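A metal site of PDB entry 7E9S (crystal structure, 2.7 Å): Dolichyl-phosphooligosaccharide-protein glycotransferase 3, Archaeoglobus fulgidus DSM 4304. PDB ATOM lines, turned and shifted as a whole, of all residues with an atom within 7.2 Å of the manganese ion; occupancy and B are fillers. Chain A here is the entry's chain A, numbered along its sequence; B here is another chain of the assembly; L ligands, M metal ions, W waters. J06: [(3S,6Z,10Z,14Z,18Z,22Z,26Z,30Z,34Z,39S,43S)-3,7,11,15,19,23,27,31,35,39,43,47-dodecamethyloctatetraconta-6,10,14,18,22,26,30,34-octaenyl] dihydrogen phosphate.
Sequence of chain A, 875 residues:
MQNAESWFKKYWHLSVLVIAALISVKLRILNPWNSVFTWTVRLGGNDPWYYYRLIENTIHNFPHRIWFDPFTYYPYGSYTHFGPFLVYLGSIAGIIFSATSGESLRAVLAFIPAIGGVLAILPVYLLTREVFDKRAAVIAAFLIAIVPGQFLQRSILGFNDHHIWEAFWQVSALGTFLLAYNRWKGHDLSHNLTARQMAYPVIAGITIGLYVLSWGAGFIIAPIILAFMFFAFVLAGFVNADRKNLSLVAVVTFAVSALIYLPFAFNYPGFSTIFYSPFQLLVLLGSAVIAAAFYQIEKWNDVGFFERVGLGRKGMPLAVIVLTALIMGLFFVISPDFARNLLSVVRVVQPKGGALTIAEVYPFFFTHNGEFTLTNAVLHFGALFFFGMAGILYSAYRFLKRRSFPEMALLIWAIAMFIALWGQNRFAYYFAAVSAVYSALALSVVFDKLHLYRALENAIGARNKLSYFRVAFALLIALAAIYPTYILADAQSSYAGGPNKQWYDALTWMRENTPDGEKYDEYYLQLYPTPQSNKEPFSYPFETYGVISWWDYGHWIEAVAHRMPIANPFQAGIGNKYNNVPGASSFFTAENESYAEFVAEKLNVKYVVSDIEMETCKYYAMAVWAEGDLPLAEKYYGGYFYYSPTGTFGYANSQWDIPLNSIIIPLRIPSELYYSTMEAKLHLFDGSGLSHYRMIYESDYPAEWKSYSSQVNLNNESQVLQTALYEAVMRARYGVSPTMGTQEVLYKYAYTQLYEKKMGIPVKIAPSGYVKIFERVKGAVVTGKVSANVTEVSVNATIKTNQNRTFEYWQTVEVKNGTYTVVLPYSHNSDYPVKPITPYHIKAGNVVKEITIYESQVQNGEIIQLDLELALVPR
The guanidinium group (NH2) of Arg 426 is in salt-bridge range of an oxygen (O65) of the ligand, 2.8 Å away.
An oxygen (O65) of the ligand is in hydrogen-bond range of a ring nitrogen (NE2) of His 162 (3.1 Å).
ND1 of His 163 sits close to NH1 of Arg 154, at 3.3 Å.
OD1 of Asp 47 lies within salt-bridge range of ND of DAB 4 of chain B.
Of the 14 residues printed, 3 come within 4 Å of the manganese ion.
Water W2 binds the manganese ion, at 2.0 Å.
The manganese ion is bound by OD2 of Asp 161 (2.1 Å).
Water W1 binds the manganese ion (2.1 Å).
NE2 of His 163 is bound to the manganese ion, at 2.3 Å.
Water W3 binds the manganese ion (2.4 Å).
The manganese ion is bound by OD2 of Asp 47 (2.4 Å).
The manganese ion has six donor atoms within binding distance.
Water W3 bridges an oxygen (O63) of the ligand and the side-chain carboxylate (OE2) of Glu 360.
Water W2 lies within hydrogen-bond range of O64 of the ligand (2.9 Å) and OD1 of Asp 161 (3.2 Å).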
ATOM      1  N   ASN A  46       5.232 -35.682   5.683  1.00  0.00           N
ATOM      2  CA  ASN A  46       5.932 -35.813   4.412  1.00  0.00           C
ATOM      3  C   ASN A  46       6.031 -34.465   3.713  1.00  0.00           C
ATOM      4  O   ASN A  46       7.119 -34.059   3.297  1.00  0.00           O
ATOM      5  CB  ASN A  46       5.215 -36.827   3.507  1.00  0.00           C
ATOM      6  CG  ASN A  46       5.376 -38.256   3.984  1.00  0.00           C
ATOM      7  OD1 ASN A  46       6.475 -38.692   4.326  1.00  0.00           O
ATOM      8  ND2 ASN A  46       4.271 -38.996   4.001  1.00  0.00           N
ATOM      9  N   ASP A  47       4.902 -33.780   3.581  1.00  0.00           N
ATOM     10  CA  ASP A  47       4.880 -32.509   2.872  1.00  0.00           C
ATOM     11  C   ASP A  47       5.771 -31.427   3.496  1.00  0.00           C
ATOM     12  O   ASP A  47       6.354 -30.642   2.723  1.00  0.00           O
ATOM     13  CB  ASP A  47       3.432 -32.005   2.750  1.00  0.00           C
ATOM     14  CG  ASP A  47       2.545 -32.986   2.003  1.00  0.00           C
ATOM     15  OD1 ASP A  47       3.051 -33.641   1.067  1.00  0.00           O
ATOM     16  OD2 ASP A  47       1.353 -33.098   2.358  1.00  0.00           O
ATOM     17  N   PRO A  48       5.909 -31.310   4.824  1.00  0.00           N
ATOM     18  CA  PRO A  48       6.902 -30.354   5.348  1.00  0.00           C
ATOM     19  C   PRO A  48       8.311 -30.602   4.825  1.00  0.00           C
ATOM     20  O   PRO A  48       9.114 -29.665   4.781  1.00  0.00           O
ATOM     21  CB  PRO A  48       6.813 -30.567   6.864  1.00  0.00           C
ATOM     22  CG  PRO A  48       5.416 -30.988   7.085  1.00  0.00           C
ATOM     23  CD  PRO A  48       5.058 -31.854   5.898  1.00  0.00           C
ATOM     24  N   TYR A  51       8.374 -28.757   1.350  1.00  0.00           N
ATOM     25  CA  TYR A  51       8.555 -27.323   1.569  1.00  0.00           C
ATOM     26  C   TYR A  51      10.014 -27.019   1.896  1.00  0.00           C
ATOM     27  O   TYR A  51      10.590 -26.067   1.371  1.00  0.00           O
ATOM     28  CB  TYR A  51       7.637 -26.834   2.677  1.00  0.00           C
ATOM     29  CG  TYR A  51       6.308 -26.298   2.178  1.00  0.00           C
ATOM     30  CD1 TYR A  51       6.250 -25.163   1.387  1.00  0.00           C
ATOM     31  CD2 TYR A  51       5.119 -26.926   2.517  1.00  0.00           C
ATOM     32  CE1 TYR A  51       5.041 -24.679   0.926  1.00  0.00           C
ATOM     33  CE2 TYR A  51       3.907 -26.447   2.064  1.00  0.00           C
ATOM     34  CZ  TYR A  51       3.867 -25.325   1.272  1.00  0.00           C
ATOM     35  OH  TYR A  51       2.667 -24.838   0.815  1.00  0.00           O
ATOM     36  N   PHE A  82       2.721 -25.944  -4.298  1.00  0.00           N
ATOM     37  CA  PHE A  82       2.922 -25.318  -3.005  1.00  0.00           C
ATOM     38  C   PHE A  82       3.034 -23.805  -3.157  1.00  0.00           C
ATOM     39  O   PHE A  82       3.720 -23.304  -4.051  1.00  0.00           O
ATOM     40  CB  PHE A  82       4.174 -25.870  -2.329  1.00  0.00           C
ATOM     41  CG  PHE A  82       3.981 -27.221  -1.676  1.00  0.00           C
ATOM     42  CD1 PHE A  82       2.817 -27.936  -1.877  1.00  0.00           C
ATOM     43  CD2 PHE A  82       4.966 -27.760  -0.873  1.00  0.00           C
ATOM     44  CE1 PHE A  82       2.641 -29.185  -1.284  1.00  0.00           C
ATOM     45  CE2 PHE A  82       4.799 -29.006  -0.275  1.00  0.00           C
ATOM     46  CZ  PHE A  82       3.633 -29.708  -0.482  1.00  0.00           C
ATOM     47  N   ARG A 154      -1.424 -30.259  12.634  1.00  0.00           N
ATOM     48  CA  ARG A 154      -0.832 -29.585  11.479  1.00  0.00           C
ATOM     49  C   ARG A 154      -0.333 -28.186  11.802  1.00  0.00           C
ATOM     50  O   ARG A 154       0.096 -27.467  10.895  1.00  0.00           O
ATOM     51  CB  ARG A 154      -1.835 -29.538  10.325  1.00  0.00           C
ATOM     52  CG  ARG A 154      -2.007 -30.877   9.642  1.00  0.00           C
ATOM     53  CD  ARG A 154      -3.302 -30.954   8.852  1.00  0.00           C
ATOM     54  NE  ARG A 154      -3.484 -32.269   8.259  1.00  0.00           N
ATOM     55  CZ  ARG A 154      -3.801 -32.489   6.981  1.00  0.00           C
ATOM     56  NH1 ARG A 154      -3.983 -31.462   6.163  1.00  0.00           N
ATOM     57  NH2 ARG A 154      -3.940 -33.721   6.539  1.00  0.00           N
ATOM     58  N   PHE A 159       5.840 -29.441  11.954  1.00  0.00           N
ATOM     59  CA  PHE A 159       4.932 -29.736  10.845  1.00  0.00           C
ATOM     60  C   PHE A 159       4.745 -28.485   9.988  1.00  0.00           C
ATOM     61  O   PHE A 159       3.665 -27.907   9.865  1.00  0.00           O
ATOM     62  CB  PHE A 159       3.605 -30.262  11.366  1.00  0.00           C
ATOM     63  CG  PHE A 159       2.925 -31.201  10.406  1.00  0.00           C
ATOM     64  CD1 PHE A 159       3.057 -32.582  10.569  1.00  0.00           C
ATOM     65  CD2 PHE A 159       2.200 -30.717   9.336  1.00  0.00           C
ATOM     66  CE1 PHE A 159       2.450 -33.446   9.685  1.00  0.00           C
ATOM     67  CE2 PHE A 159       1.586 -31.584   8.448  1.00  0.00           C
ATOM     68  CZ  PHE A 159       1.717 -32.945   8.620  1.00  0.00           C
ATOM     69  N   ASP A 161       3.828 -27.241   7.244  1.00  0.00           N
ATOM     70  CA  ASP A 161       2.963 -27.351   6.080  1.00  0.00           C
ATOM     71  C   ASP A 161       2.090 -26.110   5.991  1.00  0.00           C
ATOM     72  O   ASP A 161       2.047 -25.284   6.903  1.00  0.00           O
ATOM     73  CB  ASP A 161       2.108 -28.622   6.147  1.00  0.00           C
ATOM     74  CG  ASP A 161       1.711 -29.130   4.777  1.00  0.00           C
ATOM     75  OD1 ASP A 161       1.913 -28.394   3.790  1.00  0.00           O
ATOM     76  OD2 ASP A 161       1.190 -30.257   4.680  1.00  0.00           O
ATOM     77  N   HIS A 162       1.386 -25.977   4.866  1.00  0.00           N
ATOM     78  CA  HIS A 162       0.565 -24.796   4.612  1.00  0.00           C
ATOM     79  C   HIS A 162      -0.846 -24.910   5.149  1.00  0.00           C
ATOM     80  O   HIS A 162      -1.659 -24.013   4.905  1.00  0.00           O
ATOM     81  CB  HIS A 162       0.523 -24.504   3.103  1.00  0.00           C
ATOM     82  CG  HIS A 162      -0.061 -25.615   2.288  1.00  0.00           C
ATOM     83  ND1 HIS A 162       0.631 -26.206   1.250  1.00  0.00           N
ATOM     84  CD2 HIS A 162      -1.256 -26.240   2.345  1.00  0.00           C
ATOM     85  CE1 HIS A 162      -0.126 -27.155   0.705  1.00  0.00           C
ATOM     86  NE2 HIS A 162      -1.269 -27.193   1.361  1.00  0.00           N
ATOM     87  N   HIS A 163      -1.175 -25.979   5.876  1.00  0.00           N
ATOM     88  CA  HIS A 163      -2.544 -26.173   6.328  1.00  0.00           C
ATOM     89  C   HIS A 163      -2.918 -25.188   7.431  1.00  0.00           C
ATOM     90  O   HIS A 163      -4.063 -24.713   7.480  1.00  0.00           O
ATOM     91  CB  HIS A 163      -2.746 -27.610   6.793  1.00  0.00           C
ATOM     92  CG  HIS A 163      -2.476 -28.630   5.731  1.00  0.00           C
ATOM     93  ND1 HIS A 163      -3.220 -28.709   4.567  1.00  0.00           N
ATOM     94  CD2 HIS A 163      -1.535 -29.596   5.632  1.00  0.00           C
ATOM     95  CE1 HIS A 163      -2.753 -29.684   3.818  1.00  0.00           C
ATOM     96  NE2 HIS A 163      -1.733 -30.240   4.437  1.00  0.00           N
ATOM     97  N   GLU A 360      -5.283 -39.111   5.334  1.00  0.00           N
ATOM     98  CA  GLU A 360      -5.841 -37.780   5.552  1.00  0.00           C
ATOM     99  C   GLU A 360      -7.095 -37.495   4.739  1.00  0.00           C
ATOM    100  O   GLU A 360      -7.721 -36.457   4.936  1.00  0.00           O
ATOM    101  CB  GLU A 360      -4.791 -36.704   5.241  1.00  0.00           C
ATOM    102  CG  GLU A 360      -4.662 -36.398   3.762  1.00  0.00           C
ATOM    103  CD  GLU A 360      -3.699 -35.259   3.477  1.00  0.00           C
ATOM    104  OE1 GLU A 360      -3.063 -34.758   4.432  1.00  0.00           O
ATOM    105  OE2 GLU A 360      -3.571 -34.871   2.298  1.00  0.00           O
ATOM    106  N   ARG A 426      -9.433 -34.399   6.596  1.00  0.00           N
ATOM    107  CA  ARG A 426      -8.402 -33.374   6.711  1.00  0.00           C
ATOM    108  C   ARG A 426      -9.018 -32.003   6.964  1.00  0.00           C
ATOM    109  O   ARG A 426      -8.541 -31.246   7.808  1.00  0.00           O
ATOM    110  CB  ARG A 426      -7.517 -33.340   5.470  1.00  0.00           C
ATOM    111  CG  ARG A 426      -8.236 -33.060   4.157  1.00  0.00           C
ATOM    112  CD  ARG A 426      -7.233 -32.866   3.027  1.00  0.00           C
ATOM    113  NE  ARG A 426      -6.792 -31.479   2.912  1.00  0.00           N
ATOM    114  CZ  ARG A 426      -5.935 -31.038   1.987  1.00  0.00           C
ATOM    115  NH1 ARG A 426      -5.427 -31.885   1.095  1.00  0.00           N
ATOM    116  NH2 ARG A 426      -5.588 -29.763   1.947  1.00  0.00           N
ATOM    117  N   TYR B   3      -1.886 -37.956   8.241  1.00  0.00           N
ATOM    118  CA  TYR B   3      -1.353 -36.935   7.349  1.00  0.00           C
ATOM    119  C   TYR B   3      -1.311 -37.448   5.904  1.00  0.00           C
ATOM    120  O   TYR B   3      -1.951 -38.451   5.582  1.00  0.00           O
ATOM    121  CB  TYR B   3       0.043 -36.477   7.792  1.00  0.00           C
ATOM    122  CG  TYR B   3       1.033 -37.569   8.138  1.00  0.00           C
ATOM    123  CD1 TYR B   3       0.988 -38.212   9.368  1.00  0.00           C
ATOM    124  CD2 TYR B   3       2.038 -37.937   7.250  1.00  0.00           C
ATOM    125  CE1 TYR B   3       1.896 -39.210   9.687  1.00  0.00           C
ATOM    126  CE2 TYR B   3       2.949 -38.931   7.560  1.00  0.00           C
ATOM    127  CZ  TYR B   3       2.878 -39.564   8.786  1.00  0.00           C
ATOM    128  OH  TYR B   3       3.784 -40.549   9.099  1.00  0.00           O
ATOM    129  N   DAB B   4      -0.557 -36.766   5.043  1.00  0.00           N
ATOM    130  CA  DAB B   4      -0.444 -37.160   3.648  1.00  0.00           C
ATOM    131  C   DAB B   4       0.353 -38.489   3.431  1.00  0.00           C
ATOM    132  O   DAB B   4       1.435 -38.488   2.782  1.00  0.00           O
ATOM    133  CB  DAB B   4       0.228 -36.079   2.810  1.00  0.00           C
ATOM    134  CG  DAB B   4      -0.214 -36.119   1.346  1.00  0.00           C
ATOM    135  ND  DAB B   4       0.351 -35.102   0.486  1.00  0.00           N
HETATM  136  C10 J06 L   1     -22.466 -16.731  -7.505  1.00  0.00           C
HETATM  137  C11 J06 L   1     -23.268 -17.936  -6.916  1.00  0.00           C
HETATM  138  C12 J06 L   1     -23.255 -18.093  -5.360  1.00  0.00           C
HETATM  139  C13 J06 L   1     -22.157 -19.045  -4.893  1.00  0.00           C
HETATM  140  C14 J06 L   1     -24.640 -18.480  -4.742  1.00  0.00           C
HETATM  141  C15 J06 L   1     -25.088 -19.967  -4.586  1.00  0.00           C
HETATM  142  C19 J06 L   1     -27.952 -22.395  -5.107  1.00  0.00           C
HETATM  143  C20 J06 L   1     -28.635 -22.402  -3.748  1.00  0.00           C
HETATM  144  C16 J06 L   1     -26.610 -20.253  -4.785  1.00  0.00           C
HETATM  145  C17 J06 L   1     -27.074 -21.474  -5.568  1.00  0.00           C
HETATM  146  C18 J06 L   1     -26.479 -21.612  -6.925  1.00  0.00           C
HETATM  147  C21 J06 L   1     -29.322 -23.727  -3.287  1.00  0.00           C
HETATM  148  C22 J06 L   1     -30.331 -23.660  -2.132  1.00  0.00           C
HETATM  149  C23 J06 L   1     -31.748 -23.450  -2.546  1.00  0.00           C
HETATM  150  C01 J06 L   1     -17.526 -17.158 -12.437  1.00  0.00           C
HETATM  151  C02 J06 L   1     -16.629 -16.735 -11.267  1.00  0.00           C
HETATM  152  C03 J06 L   1     -16.676 -15.214 -11.199  1.00  0.00           C
HETATM  153  C04 J06 L   1     -17.036 -17.401  -9.927  1.00  0.00           C
HETATM  154  C05 J06 L   1     -18.525 -17.226  -9.539  1.00  0.00           C
HETATM  155  C06 J06 L   1     -19.006 -18.194  -8.425  1.00  0.00           C
HETATM  156  C07 J06 L   1     -20.559 -18.391  -8.320  1.00  0.00           C
HETATM  157  C08 J06 L   1     -20.973 -19.499  -9.297  1.00  0.00           C
HETATM  158  C09 J06 L   1     -21.410 -17.080  -8.589  1.00  0.00           C
HETATM  159  C24 J06 L   1     -30.017 -23.762  -0.819  1.00  0.00           C
HETATM  160  C25 J06 L   1     -28.641 -23.981  -0.188  1.00  0.00           C
HETATM  161  C26 J06 L   1     -28.452 -23.387   1.260  1.00  0.00           C
HETATM  162  C27 J06 L   1     -27.543 -24.049   2.315  1.00  0.00           C
HETATM  163  C28 J06 L   1     -28.188 -25.069   3.192  1.00  0.00           C
HETATM  164  C29 J06 L   1     -26.227 -23.764   2.454  1.00  0.00           C
HETATM  165  C30 J06 L   1     -25.369 -22.774   1.669  1.00  0.00           C
HETATM  166  C31 J06 L   1     -24.339 -23.329   0.624  1.00  0.00           C
HETATM  167  C32 J06 L   1     -23.884 -22.469  -0.566  1.00  0.00           C
HETATM  168  C33 J06 L   1     -24.969 -21.833  -1.365  1.00  0.00           C
HETATM  169  C34 J06 L   1     -22.598 -22.295  -0.916  1.00  0.00           C
HETATM  170  C35 J06 L   1     -21.350 -22.859  -0.247  1.00  0.00           C
HETATM  171  C36 J06 L   1     -20.531 -23.915  -1.056  1.00  0.00           C
HETATM  172  C37 J06 L   1     -20.985 -25.376  -1.218  1.00  0.00           C
HETATM  173  C38 J06 L   1     -22.360 -25.618  -1.744  1.00  0.00           C
HETATM  174  C39 J06 L   1     -20.185 -26.418  -0.912  1.00  0.00           C
HETATM  175  C40 J06 L   1     -18.782 -26.331  -0.374  1.00  0.00           C
HETATM  176  C41 J06 L   1     -18.020 -27.631  -0.036  1.00  0.00           C
HETATM  177  C42 J06 L   1     -17.418 -28.358  -1.211  1.00  0.00           C
HETATM  178  C43 J06 L   1     -18.371 -29.305  -1.881  1.00  0.00           C
HETATM  179  C44 J06 L   1     -16.172 -28.228  -1.679  1.00  0.00           C
HETATM  180  C45 J06 L   1     -15.098 -27.335  -1.148  1.00  0.00           C
HETATM  181  C46 J06 L   1     -14.018 -28.020  -0.281  1.00  0.00           C
HETATM  182  C47 J06 L   1     -12.752 -27.242  -0.025  1.00  0.00           C
HETATM  183  C48 J06 L   1     -12.654 -26.637   1.340  1.00  0.00           C
HETATM  184  C49 J06 L   1     -11.764 -27.060  -0.919  1.00  0.00           C
HETATM  185  C50 J06 L   1     -11.723 -27.600  -2.320  1.00  0.00           C
HETATM  186  C51 J06 L   1     -10.962 -26.756  -3.377  1.00  0.00           C
HETATM  187  C52 J06 L   1     -10.337 -27.431  -4.563  1.00  0.00           C
HETATM  188  C53 J06 L   1     -10.937 -27.069  -5.888  1.00  0.00           C
HETATM  189  C54 J06 L   1      -9.313 -28.312  -4.521  1.00  0.00           C
HETATM  190  C55 J06 L   1      -8.549 -28.827  -3.324  1.00  0.00           C
HETATM  191  C56 J06 L   1      -7.533 -29.969  -3.593  1.00  0.00           C
HETATM  192  C57 J06 L   1      -6.822 -30.557  -2.334  1.00  0.00           C
HETATM  193  C58 J06 L   1      -7.719 -30.393  -1.102  1.00  0.00           C
HETATM  194  C59 J06 L   1      -5.447 -29.906  -2.011  1.00  0.00           C
HETATM  195  C60 J06 L   1      -4.191 -30.821  -2.352  1.00  0.00           C
HETATM  196  O61 J06 L   1      -3.053 -30.178  -2.008  1.00  0.00           O
HETATM  197  O63 J06 L   1      -2.597 -31.875  -0.065  1.00  0.00           O
HETATM  198  O64 J06 L   1      -0.935 -29.965  -0.503  1.00  0.00           O
HETATM  199  O65 J06 L   1      -3.258 -29.442   0.469  1.00  0.00           O
HETATM  200  P62 J06 L   1      -2.374 -30.403  -0.305  1.00  0.00           P
HETATM  201 MN    MN M   1      -0.076 -31.635   3.695  1.00  0.00          MN
HETATM  202  O   HOH W   1      -0.621 -32.817   5.370  1.00  0.00           O
HETATM  203  O   HOH W   2       0.374 -30.603   1.993  1.00  0.00           O
HETATM  204  O   HOH W   3      -1.868 -32.559   2.384  1.00  0.00           O
